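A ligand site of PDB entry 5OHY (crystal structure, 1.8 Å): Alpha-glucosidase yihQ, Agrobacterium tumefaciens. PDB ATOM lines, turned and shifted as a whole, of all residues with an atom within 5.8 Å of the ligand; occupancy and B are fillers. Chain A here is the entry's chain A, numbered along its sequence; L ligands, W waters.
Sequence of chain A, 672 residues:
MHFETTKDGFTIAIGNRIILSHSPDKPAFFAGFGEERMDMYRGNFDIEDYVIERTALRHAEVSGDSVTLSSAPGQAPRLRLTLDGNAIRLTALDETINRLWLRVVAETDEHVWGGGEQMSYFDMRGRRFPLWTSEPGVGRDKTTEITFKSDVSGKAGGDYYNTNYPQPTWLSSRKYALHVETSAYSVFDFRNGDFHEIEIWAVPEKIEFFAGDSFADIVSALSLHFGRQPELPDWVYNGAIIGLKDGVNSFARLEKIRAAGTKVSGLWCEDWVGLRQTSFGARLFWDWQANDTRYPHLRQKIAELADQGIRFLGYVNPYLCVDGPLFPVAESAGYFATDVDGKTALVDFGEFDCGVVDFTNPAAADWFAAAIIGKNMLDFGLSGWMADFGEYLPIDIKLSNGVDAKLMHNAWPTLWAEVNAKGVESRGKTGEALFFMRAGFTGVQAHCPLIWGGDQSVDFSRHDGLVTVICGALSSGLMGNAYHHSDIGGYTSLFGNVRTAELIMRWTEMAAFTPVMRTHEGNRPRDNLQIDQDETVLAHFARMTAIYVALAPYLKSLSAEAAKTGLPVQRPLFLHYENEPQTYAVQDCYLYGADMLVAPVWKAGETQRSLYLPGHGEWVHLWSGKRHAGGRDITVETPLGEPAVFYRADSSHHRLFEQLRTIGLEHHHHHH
O4 of the ligand lies within hydrogen-bond range of NE2 of His 520.
SD of Met 386 lies close to O4 of the ligand (3.6 Å).
An oxygen (O2) of the ligand sits at hydrogen-bond distance from the backbone NH (N) of Leu 284, at 3.0 Å.
NH2 of Arg 283 lies within salt-bridge range of O1 of the ligand (2.9 Å).
The side-chain carboxylate (OD2) of Asp 388 lies within salt-bridge range of a nitrogen (N1) of the ligand.
The guanidinium group of Arg 438 sits close to a nitrogen (N1) of the ligand (3.4 Å).
The indole nitrogen (NE1) of Trp 286 is in hydrogen-bond range of an oxygen (O2) of the ligand.
OE1 of Glu 270 lies within hydrogen-bond range of O5 of the ligand, at 2.5 Å.
OD1 of Asp 388 is in salt-bridge range of NE of Arg 438 (3.1 Å).
The side-chain carboxylate (OD2) of Asp 455 lies within salt-bridge range of the guanidinium group (NH1) of Arg 438, 3.5 Å away.
NZ of Lys 245 lies within salt-bridge range of OE2 of Glu 270 (2.6 Å).
The backbone NH (N) of Gly 522 is in hydrogen-bond range of a ring nitrogen (ND1) of His 520 (3.0 Å).
The side-chain amino group (NZ) of Lys 245 lies within hydrogen-bond range of the backbone carbonyl oxygen (O) of Ala 282, at 2.8 Å.
OD2 of Asp 388 sits at hydrogen-bond distance from OH of Tyr 315 (2.6 Å).
Residues that only touch the ligand: Ala 282, Tyr 315, Phe 389, Asp 455 and Tyr 491.
Hydrophobic or aromatic side chains within 4 Å of the ligand: Leu 284, Trp 286, Met 386, Phe 389, Tyr 491 and His 520.
13 residues have an atom within 4 Å of the ligand: Glu 270, Ala 282, Arg 283, Leu 284, Trp 286, Tyr 315, Met 386, Asp 388, Phe 389, Arg 438, Asp 455, Tyr 491 and His 520.
The nearest printed residue that does not touch the ligand is Trp 452 (4.1 Å).
Water W2 lies within hydrogen-bond range of O5 of the ligand, OH of Tyr 491, NZ of Lys 245 and OE2 of Glu 270.
Water W1 lies within hydrogen-bond range of the side-chain carboxylate (OD2) of Asp 487 (2.6 Å), an oxygen (O4) of the ligand (2.7 Å), the side-chain carboxylate (OD1) of Asp 455 (2.8 Å) and the indole nitrogen (NE1) of Trp 452 (3.1 Å).
Water W3 bridges OH of Tyr 491 (2.7 Å) and O3 of the ligand (3.2 Å).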
ATOM      1  N   LYS A 245      24.747  19.757  21.485  1.00  0.00           N
ATOM      2  CA  LYS A 245      23.925  18.608  21.029  1.00  0.00           C
ATOM      3  C   LYS A 245      23.316  18.927  19.700  1.00  0.00           C
ATOM      4  O   LYS A 245      22.138  18.647  19.440  1.00  0.00           O
ATOM      5  CB  LYS A 245      22.895  18.241  22.133  1.00  0.00           C
ATOM      6  CG  LYS A 245      22.057  19.419  22.591  1.00  0.00           C
ATOM      7  CD  LYS A 245      21.200  19.045  23.823  1.00  0.00           C
ATOM      8  CE  LYS A 245      20.007  18.162  23.491  1.00  0.00           C
ATOM      9  NZ  LYS A 245      19.324  17.704  24.771  1.00  0.00           N
ATOM     10  N   TRP A 268      31.725  17.828  24.644  1.00  0.00           N
ATOM     11  CA  TRP A 268      30.841  16.824  25.204  1.00  0.00           C
ATOM     12  C   TRP A 268      29.540  16.882  24.345  1.00  0.00           C
ATOM     13  O   TRP A 268      28.815  17.905  24.365  1.00  0.00           O
ATOM     14  CB  TRP A 268      30.494  17.148  26.664  1.00  0.00           C
ATOM     15  CG  TRP A 268      29.334  16.358  27.186  1.00  0.00           C
ATOM     16  CD1 TRP A 268      29.197  15.035  27.149  1.00  0.00           C
ATOM     17  CD2 TRP A 268      28.159  16.890  27.770  1.00  0.00           C
ATOM     18  NE1 TRP A 268      28.005  14.649  27.741  1.00  0.00           N
ATOM     19  CE2 TRP A 268      27.317  15.784  28.072  1.00  0.00           C
ATOM     20  CE3 TRP A 268      27.707  18.170  28.027  1.00  0.00           C
ATOM     21  CZ2 TRP A 268      26.065  15.941  28.631  1.00  0.00           C
ATOM     22  CZ3 TRP A 268      26.426  18.320  28.572  1.00  0.00           C
ATOM     23  CH2 TRP A 268      25.628  17.205  28.850  1.00  0.00           C
ATOM     24  N   GLU A 270      26.222  14.929  23.978  1.00  0.00           N
ATOM     25  CA  GLU A 270      25.354  13.880  24.486  1.00  0.00           C
ATOM     26  C   GLU A 270      24.563  13.189  23.349  1.00  0.00           C
ATOM     27  O   GLU A 270      24.151  12.030  23.469  1.00  0.00           O
ATOM     28  CB  GLU A 270      24.424  14.389  25.602  1.00  0.00           C
ATOM     29  CG  GLU A 270      23.478  15.483  25.177  1.00  0.00           C
ATOM     30  CD  GLU A 270      22.368  15.788  26.235  1.00  0.00           C
ATOM     31  OE1 GLU A 270      22.503  15.370  27.386  1.00  0.00           O
ATOM     32  OE2 GLU A 270      21.374  16.456  25.882  1.00  0.00           O
ATOM     33  N   ALA A 282      14.251  18.073  23.270  1.00  0.00           N
ATOM     34  CA  ALA A 282      15.288  17.459  22.407  1.00  0.00           C
ATOM     35  C   ALA A 282      15.901  16.317  23.199  1.00  0.00           C
ATOM     36  O   ALA A 282      16.893  16.505  23.945  1.00  0.00           O
ATOM     37  CB  ALA A 282      16.347  18.481  22.071  1.00  0.00           C
ATOM     38  N   ARG A 283      15.248  15.139  23.111  1.00  0.00           N
ATOM     39  CA  ARG A 283      15.782  14.009  23.838  1.00  0.00           C
ATOM     40  C   ARG A 283      16.826  13.254  23.029  1.00  0.00           C
ATOM     41  O   ARG A 283      17.098  13.639  21.881  1.00  0.00           O
ATOM     42  CB  ARG A 283      14.628  13.105  24.276  1.00  0.00           C
ATOM     43  CG  ARG A 283      13.560  13.954  25.065  1.00  0.00           C
ATOM     44  CD  ARG A 283      12.844  13.243  26.117  1.00  0.00           C
ATOM     45  NE  ARG A 283      13.655  12.670  27.188  1.00  0.00           N
ATOM     46  CZ  ARG A 283      13.134  11.899  28.128  1.00  0.00           C
ATOM     47  NH1 ARG A 283      11.807  11.603  28.032  1.00  0.00           N
ATOM     48  NH2 ARG A 283      13.879  11.431  29.110  1.00  0.00           N
ATOM     49  N   LEU A 284      17.433  12.272  23.623  1.00  0.00           N
ATOM     50  CA  LEU A 284      18.484  11.452  22.966  1.00  0.00           C
ATOM     51  C   LEU A 284      17.882  10.076  22.625  1.00  0.00           C
ATOM     52  O   LEU A 284      16.854   9.646  23.216  1.00  0.00           O
ATOM     53  CB  LEU A 284      19.658  11.238  23.907  1.00  0.00           C
ATOM     54  CG  LEU A 284      20.205  12.529  24.577  1.00  0.00           C
ATOM     55  CD1 LEU A 284      21.343  12.205  25.557  1.00  0.00           C
ATOM     56  CD2 LEU A 284      20.648  13.503  23.525  1.00  0.00           C
ATOM     57  N   PHE A 285      18.507   9.383  21.653  1.00  0.00           N
ATOM     58  CA  PHE A 285      18.206   8.027  21.320  1.00  0.00           C
ATOM     59  C   PHE A 285      18.966   7.059  22.198  1.00  0.00           C
ATOM     60  O   PHE A 285      20.211   6.938  22.086  1.00  0.00           O
ATOM     61  CB  PHE A 285      18.484   7.791  19.834  1.00  0.00           C
ATOM     62  CG  PHE A 285      17.904   6.496  19.314  1.00  0.00           C
ATOM     63  CD1 PHE A 285      16.562   6.435  19.025  1.00  0.00           C
ATOM     64  CD2 PHE A 285      18.686   5.387  19.100  1.00  0.00           C
ATOM     65  CE1 PHE A 285      15.983   5.193  18.613  1.00  0.00           C
ATOM     66  CE2 PHE A 285      18.104   4.163  18.637  1.00  0.00           C
ATOM     67  CZ  PHE A 285      16.749   4.066  18.400  1.00  0.00           C
ATOM     68  N   TRP A 286      18.292   6.323  23.073  1.00  0.00           N
ATOM     69  CA  TRP A 286      18.935   5.550  24.130  1.00  0.00           C
ATOM     70  C   TRP A 286      19.416   4.161  23.682  1.00  0.00           C
ATOM     71  O   TRP A 286      18.920   3.096  24.134  1.00  0.00           O
ATOM     72  CB  TRP A 286      18.053   5.442  25.376  1.00  0.00           C
ATOM     73  CG  TRP A 286      17.812   6.754  26.081  1.00  0.00           C
ATOM     74  CD1 TRP A 286      18.092   8.004  25.639  1.00  0.00           C
ATOM     75  CD2 TRP A 286      17.188   6.900  27.350  1.00  0.00           C
ATOM     76  NE1 TRP A 286      17.674   8.921  26.563  1.00  0.00           N
ATOM     77  CE2 TRP A 286      17.139   8.263  27.648  1.00  0.00           C
ATOM     78  CE3 TRP A 286      16.636   5.999  28.246  1.00  0.00           C
ATOM     79  CZ2 TRP A 286      16.551   8.760  28.789  1.00  0.00           C
ATOM     80  CZ3 TRP A 286      16.048   6.481  29.404  1.00  0.00           C
ATOM     81  CH2 TRP A 286      16.033   7.838  29.655  1.00  0.00           C
ATOM     82  N   TYR A 315      27.693  10.175  26.447  1.00  0.00           N
ATOM     83  CA  TYR A 315      26.502  10.056  27.289  1.00  0.00           C
ATOM     84  C   TYR A 315      26.081   8.570  27.256  1.00  0.00           C
ATOM     85  O   TYR A 315      26.061   7.967  26.187  1.00  0.00           O
ATOM     86  CB  TYR A 315      25.331  10.914  26.768  1.00  0.00           C
ATOM     87  CG  TYR A 315      24.062  10.719  27.569  1.00  0.00           C
ATOM     88  CD1 TYR A 315      23.280   9.581  27.371  1.00  0.00           C
ATOM     89  CD2 TYR A 315      23.706  11.596  28.599  1.00  0.00           C
ATOM     90  CE1 TYR A 315      22.170   9.336  28.178  1.00  0.00           C
ATOM     91  CE2 TYR A 315      22.562  11.360  29.387  1.00  0.00           C
ATOM     92  CZ  TYR A 315      21.798  10.241  29.142  1.00  0.00           C
ATOM     93  OH  TYR A 315      20.698   9.952  29.909  1.00  0.00           O
ATOM     94  N   PHE A 352       9.027   7.347  25.185  1.00  0.00           N
ATOM     95  CA  PHE A 352       9.521   6.026  24.785  1.00  0.00           C
ATOM     96  C   PHE A 352       9.662   5.183  26.038  1.00  0.00           C
ATOM     97  O   PHE A 352       9.758   5.660  27.146  1.00  0.00           O
ATOM     98  CB  PHE A 352      10.909   6.136  24.004  1.00  0.00           C
ATOM     99  CG  PHE A 352      11.935   6.990  24.770  1.00  0.00           C
ATOM    100  CD1 PHE A 352      12.745   6.451  25.727  1.00  0.00           C
ATOM    101  CD2 PHE A 352      12.025   8.300  24.474  1.00  0.00           C
ATOM    102  CE1 PHE A 352      13.654   7.254  26.429  1.00  0.00           C
ATOM    103  CE2 PHE A 352      12.901   9.160  25.178  1.00  0.00           C
ATOM    104  CZ  PHE A 352      13.742   8.599  26.153  1.00  0.00           C
ATOM    105  N   MET A 386      28.880  11.699  30.496  1.00  0.00           N
ATOM    106  CA  MET A 386      27.768  11.738  31.501  1.00  0.00           C
ATOM    107  C   MET A 386      27.268  10.285  31.655  1.00  0.00           C
ATOM    108  O   MET A 386      26.845   9.666  30.685  1.00  0.00           O
ATOM    109  CB  MET A 386      26.622  12.641  30.997  1.00  0.00           C
ATOM    110  CG  MET A 386      25.454  12.773  31.975  1.00  0.00           C
ATOM    111  SD  MET A 386      24.212  13.911  31.364  1.00  0.00           S
ATOM    112  CE  MET A 386      24.900  15.477  31.957  1.00  0.00           C
ATOM    113  N   ASP A 388      24.446   8.737  33.379  1.00  0.00           N
ATOM    114  CA  ASP A 388      23.192   9.340  33.861  1.00  0.00           C
ATOM    115  C   ASP A 388      22.261   8.287  34.464  1.00  0.00           C
ATOM    116  O   ASP A 388      22.469   7.071  34.348  1.00  0.00           O
ATOM    117  CB  ASP A 388      22.497   9.971  32.662  1.00  0.00           C
ATOM    118  CG  ASP A 388      21.426  10.993  33.054  1.00  0.00           C
ATOM    119  OD1 ASP A 388      21.317  11.411  34.238  1.00  0.00           O
ATOM    120  OD2 ASP A 388      20.645  11.365  32.141  1.00  0.00           O
ATOM    121  N   PHE A 389      21.231   8.790  35.133  1.00  0.00           N
ATOM    122  CA  PHE A 389      20.193   7.985  35.766  1.00  0.00           C
ATOM    123  C   PHE A 389      20.709   7.057  36.841  1.00  0.00           C
ATOM    124  O   PHE A 389      21.767   7.294  37.441  1.00  0.00           O
ATOM    125  CB  PHE A 389      19.334   7.286  34.667  1.00  0.00           C
ATOM    126  CG  PHE A 389      18.447   8.213  33.879  1.00  0.00           C
ATOM    127  CD1 PHE A 389      17.112   8.517  34.312  1.00  0.00           C
ATOM    128  CD2 PHE A 389      18.866   8.778  32.688  1.00  0.00           C
ATOM    129  CE1 PHE A 389      16.308   9.347  33.519  1.00  0.00           C
ATOM    130  CE2 PHE A 389      18.075   9.559  31.937  1.00  0.00           C
ATOM    131  CZ  PHE A 389      16.794   9.895  32.347  1.00  0.00           C
ATOM    132  N   ARG A 438      24.920  11.857  38.410  1.00  0.00           N
ATOM    133  CA  ARG A 438      24.033  12.664  39.231  1.00  0.00           C
ATOM    134  C   ARG A 438      23.415  11.835  40.350  1.00  0.00           C
ATOM    135  O   ARG A 438      23.032  12.400  41.375  1.00  0.00           O
ATOM    136  CB  ARG A 438      22.915  13.334  38.370  1.00  0.00           C
ATOM    137  CG  ARG A 438      21.852  12.328  37.844  1.00  0.00           C
ATOM    138  CD  ARG A 438      20.792  13.013  37.011  1.00  0.00           C
ATOM    139  NE  ARG A 438      19.691  12.099  36.753  1.00  0.00           N
ATOM    140  CZ  ARG A 438      18.610  12.408  36.050  1.00  0.00           C
ATOM    141  NH1 ARG A 438      18.503  13.613  35.423  1.00  0.00           N
ATOM    142  NH2 ARG A 438      17.657  11.472  35.917  1.00  0.00           N
ATOM    143  N   TRP A 452      27.938  15.423  39.357  1.00  0.00           N
ATOM    144  CA  TRP A 452      27.330  16.674  38.932  1.00  0.00           C
ATOM    145  C   TRP A 452      25.967  16.824  39.610  1.00  0.00           C
ATOM    146  O   TRP A 452      25.335  15.819  40.020  1.00  0.00           O
ATOM    147  CB  TRP A 452      27.249  16.875  37.427  1.00  0.00           C
ATOM    148  CG  TRP A 452      25.941  16.691  36.688  1.00  0.00           C
ATOM    149  CD1 TRP A 452      25.057  17.668  36.335  1.00  0.00           C
ATOM    150  CD2 TRP A 452      25.433  15.496  36.165  1.00  0.00           C
ATOM    151  NE1 TRP A 452      24.037  17.158  35.625  1.00  0.00           N
ATOM    152  CE2 TRP A 452      24.215  15.810  35.528  1.00  0.00           C
ATOM    153  CE3 TRP A 452      25.892  14.162  36.154  1.00  0.00           C
ATOM    154  CZ2 TRP A 452      23.425  14.813  34.861  1.00  0.00           C
ATOM    155  CZ3 TRP A 452      25.120  13.195  35.534  1.00  0.00           C
ATOM    156  CH2 TRP A 452      23.903  13.525  34.880  1.00  0.00           C
ATOM    157  N   ASP A 455      19.804  18.027  37.313  1.00  0.00           N
ATOM    158  CA  ASP A 455      19.049  19.038  36.619  1.00  0.00           C
ATOM    159  C   ASP A 455      18.586  20.174  37.574  1.00  0.00           C
ATOM    160  O   ASP A 455      17.788  19.928  38.491  1.00  0.00           O
ATOM    161  CB  ASP A 455      17.777  18.459  35.984  1.00  0.00           C
ATOM    162  CG  ASP A 455      18.026  17.306  35.009  1.00  0.00           C
ATOM    163  OD1 ASP A 455      19.185  16.996  34.645  1.00  0.00           O
ATOM    164  OD2 ASP A 455      16.977  16.698  34.617  1.00  0.00           O
ATOM    165  N   ASP A 487      25.752  21.839  35.541  1.00  0.00           N
ATOM    166  CA  ASP A 487      25.513  22.358  34.217  1.00  0.00           C
ATOM    167  C   ASP A 487      25.560  23.890  34.255  1.00  0.00           C
ATOM    168  O   ASP A 487      24.709  24.528  34.909  1.00  0.00           O
ATOM    169  CB  ASP A 487      24.110  21.963  33.692  1.00  0.00           C
ATOM    170  CG  ASP A 487      23.875  20.457  33.715  1.00  0.00           C
ATOM    171  OD1 ASP A 487      24.754  19.646  33.280  1.00  0.00           O
ATOM    172  OD2 ASP A 487      22.741  20.086  34.137  1.00  0.00           O
ATOM    173  N   TYR A 491      19.591  23.365  33.538  1.00  0.00           N
ATOM    174  CA  TYR A 491      19.079  22.397  32.558  1.00  0.00           C
ATOM    175  C   TYR A 491      17.595  22.603  32.176  1.00  0.00           C
ATOM    176  O   TYR A 491      17.271  22.766  31.003  1.00  0.00           O
ATOM    177  CB  TYR A 491      19.281  20.985  33.107  1.00  0.00           C
ATOM    178  CG  TYR A 491      18.710  19.956  32.165  1.00  0.00           C
ATOM    179  CD1 TYR A 491      19.397  19.545  31.028  1.00  0.00           C
ATOM    180  CD2 TYR A 491      17.403  19.449  32.374  1.00  0.00           C
ATOM    181  CE1 TYR A 491      18.829  18.659  30.124  1.00  0.00           C
ATOM    182  CE2 TYR A 491      16.841  18.554  31.498  1.00  0.00           C
ATOM    183  CZ  TYR A 491      17.543  18.140  30.353  1.00  0.00           C
ATOM    184  OH  TYR A 491      16.997  17.271  29.435  1.00  0.00           O
ATOM    185  N   HIS A 520      25.960  23.044  28.694  1.00  0.00           N
ATOM    186  CA  HIS A 520      24.877  22.109  28.327  1.00  0.00           C
ATOM    187  C   HIS A 520      23.823  22.926  27.607  1.00  0.00           C
ATOM    188  O   HIS A 520      23.393  24.006  28.082  1.00  0.00           O
ATOM    189  CB  HIS A 520      24.285  21.464  29.612  1.00  0.00           C
ATOM    190  CG  HIS A 520      23.447  20.237  29.393  1.00  0.00           C
ATOM    191  ND1 HIS A 520      22.846  19.934  28.204  1.00  0.00           N
ATOM    192  CD2 HIS A 520      23.074  19.261  30.266  1.00  0.00           C
ATOM    193  CE1 HIS A 520      22.160  18.770  28.336  1.00  0.00           C
ATOM    194  NE2 HIS A 520      22.291  18.350  29.581  1.00  0.00           N
ATOM    195  N   GLY A 522      20.815  21.958  27.168  1.00  0.00           N
ATOM    196  CA  GLY A 522      19.567  21.694  27.945  1.00  0.00           C
ATOM    197  C   GLY A 522      18.498  20.900  27.177  1.00  0.00           C
ATOM    198  O   GLY A 522      18.747  20.295  26.102  1.00  0.00           O
HETATM  199  O1  LIG L   1      16.676  12.268  28.815  1.00  0.00           O
HETATM  200  S1  LIG L   1      17.380  12.915  27.603  1.00  0.00           S
HETATM  201  O2  LIG L   1      17.582  11.904  26.608  1.00  0.00           O
HETATM  202  O3  LIG L   1      16.766  14.084  27.086  1.00  0.00           O
HETATM  203  C1  LIG L   1      18.978  13.342  28.232  1.00  0.00           C
HETATM  204  C2  LIG L   1      19.064  14.141  29.526  1.00  0.00           C
HETATM  205  C3  LIG L   1      18.884  13.176  30.696  1.00  0.00           C
HETATM  206  N1  LIG L   1      19.075  13.674  32.050  1.00  0.00           N
HETATM  207  C4  LIG L   1      20.296  14.537  32.167  1.00  0.00           C
HETATM  208  C5  LIG L   1      20.429  15.610  31.092  1.00  0.00           C
HETATM  209  O4  LIG L   1      21.630  16.357  31.303  1.00  0.00           O
HETATM  210  C6  LIG L   1      20.348  14.987  29.692  1.00  0.00           C
HETATM  211  O5  LIG L   1      20.408  16.003  28.663  1.00  0.00           O
HETATM  212  O   HOH W   1      21.683  17.779  33.644  1.00  0.00           O
HETATM  213  O   HOH W   2      18.341  16.594  27.373  1.00  0.00           O
HETATM  214  O   HOH W   3      14.782  15.819  28.874  1.00  0.00           O
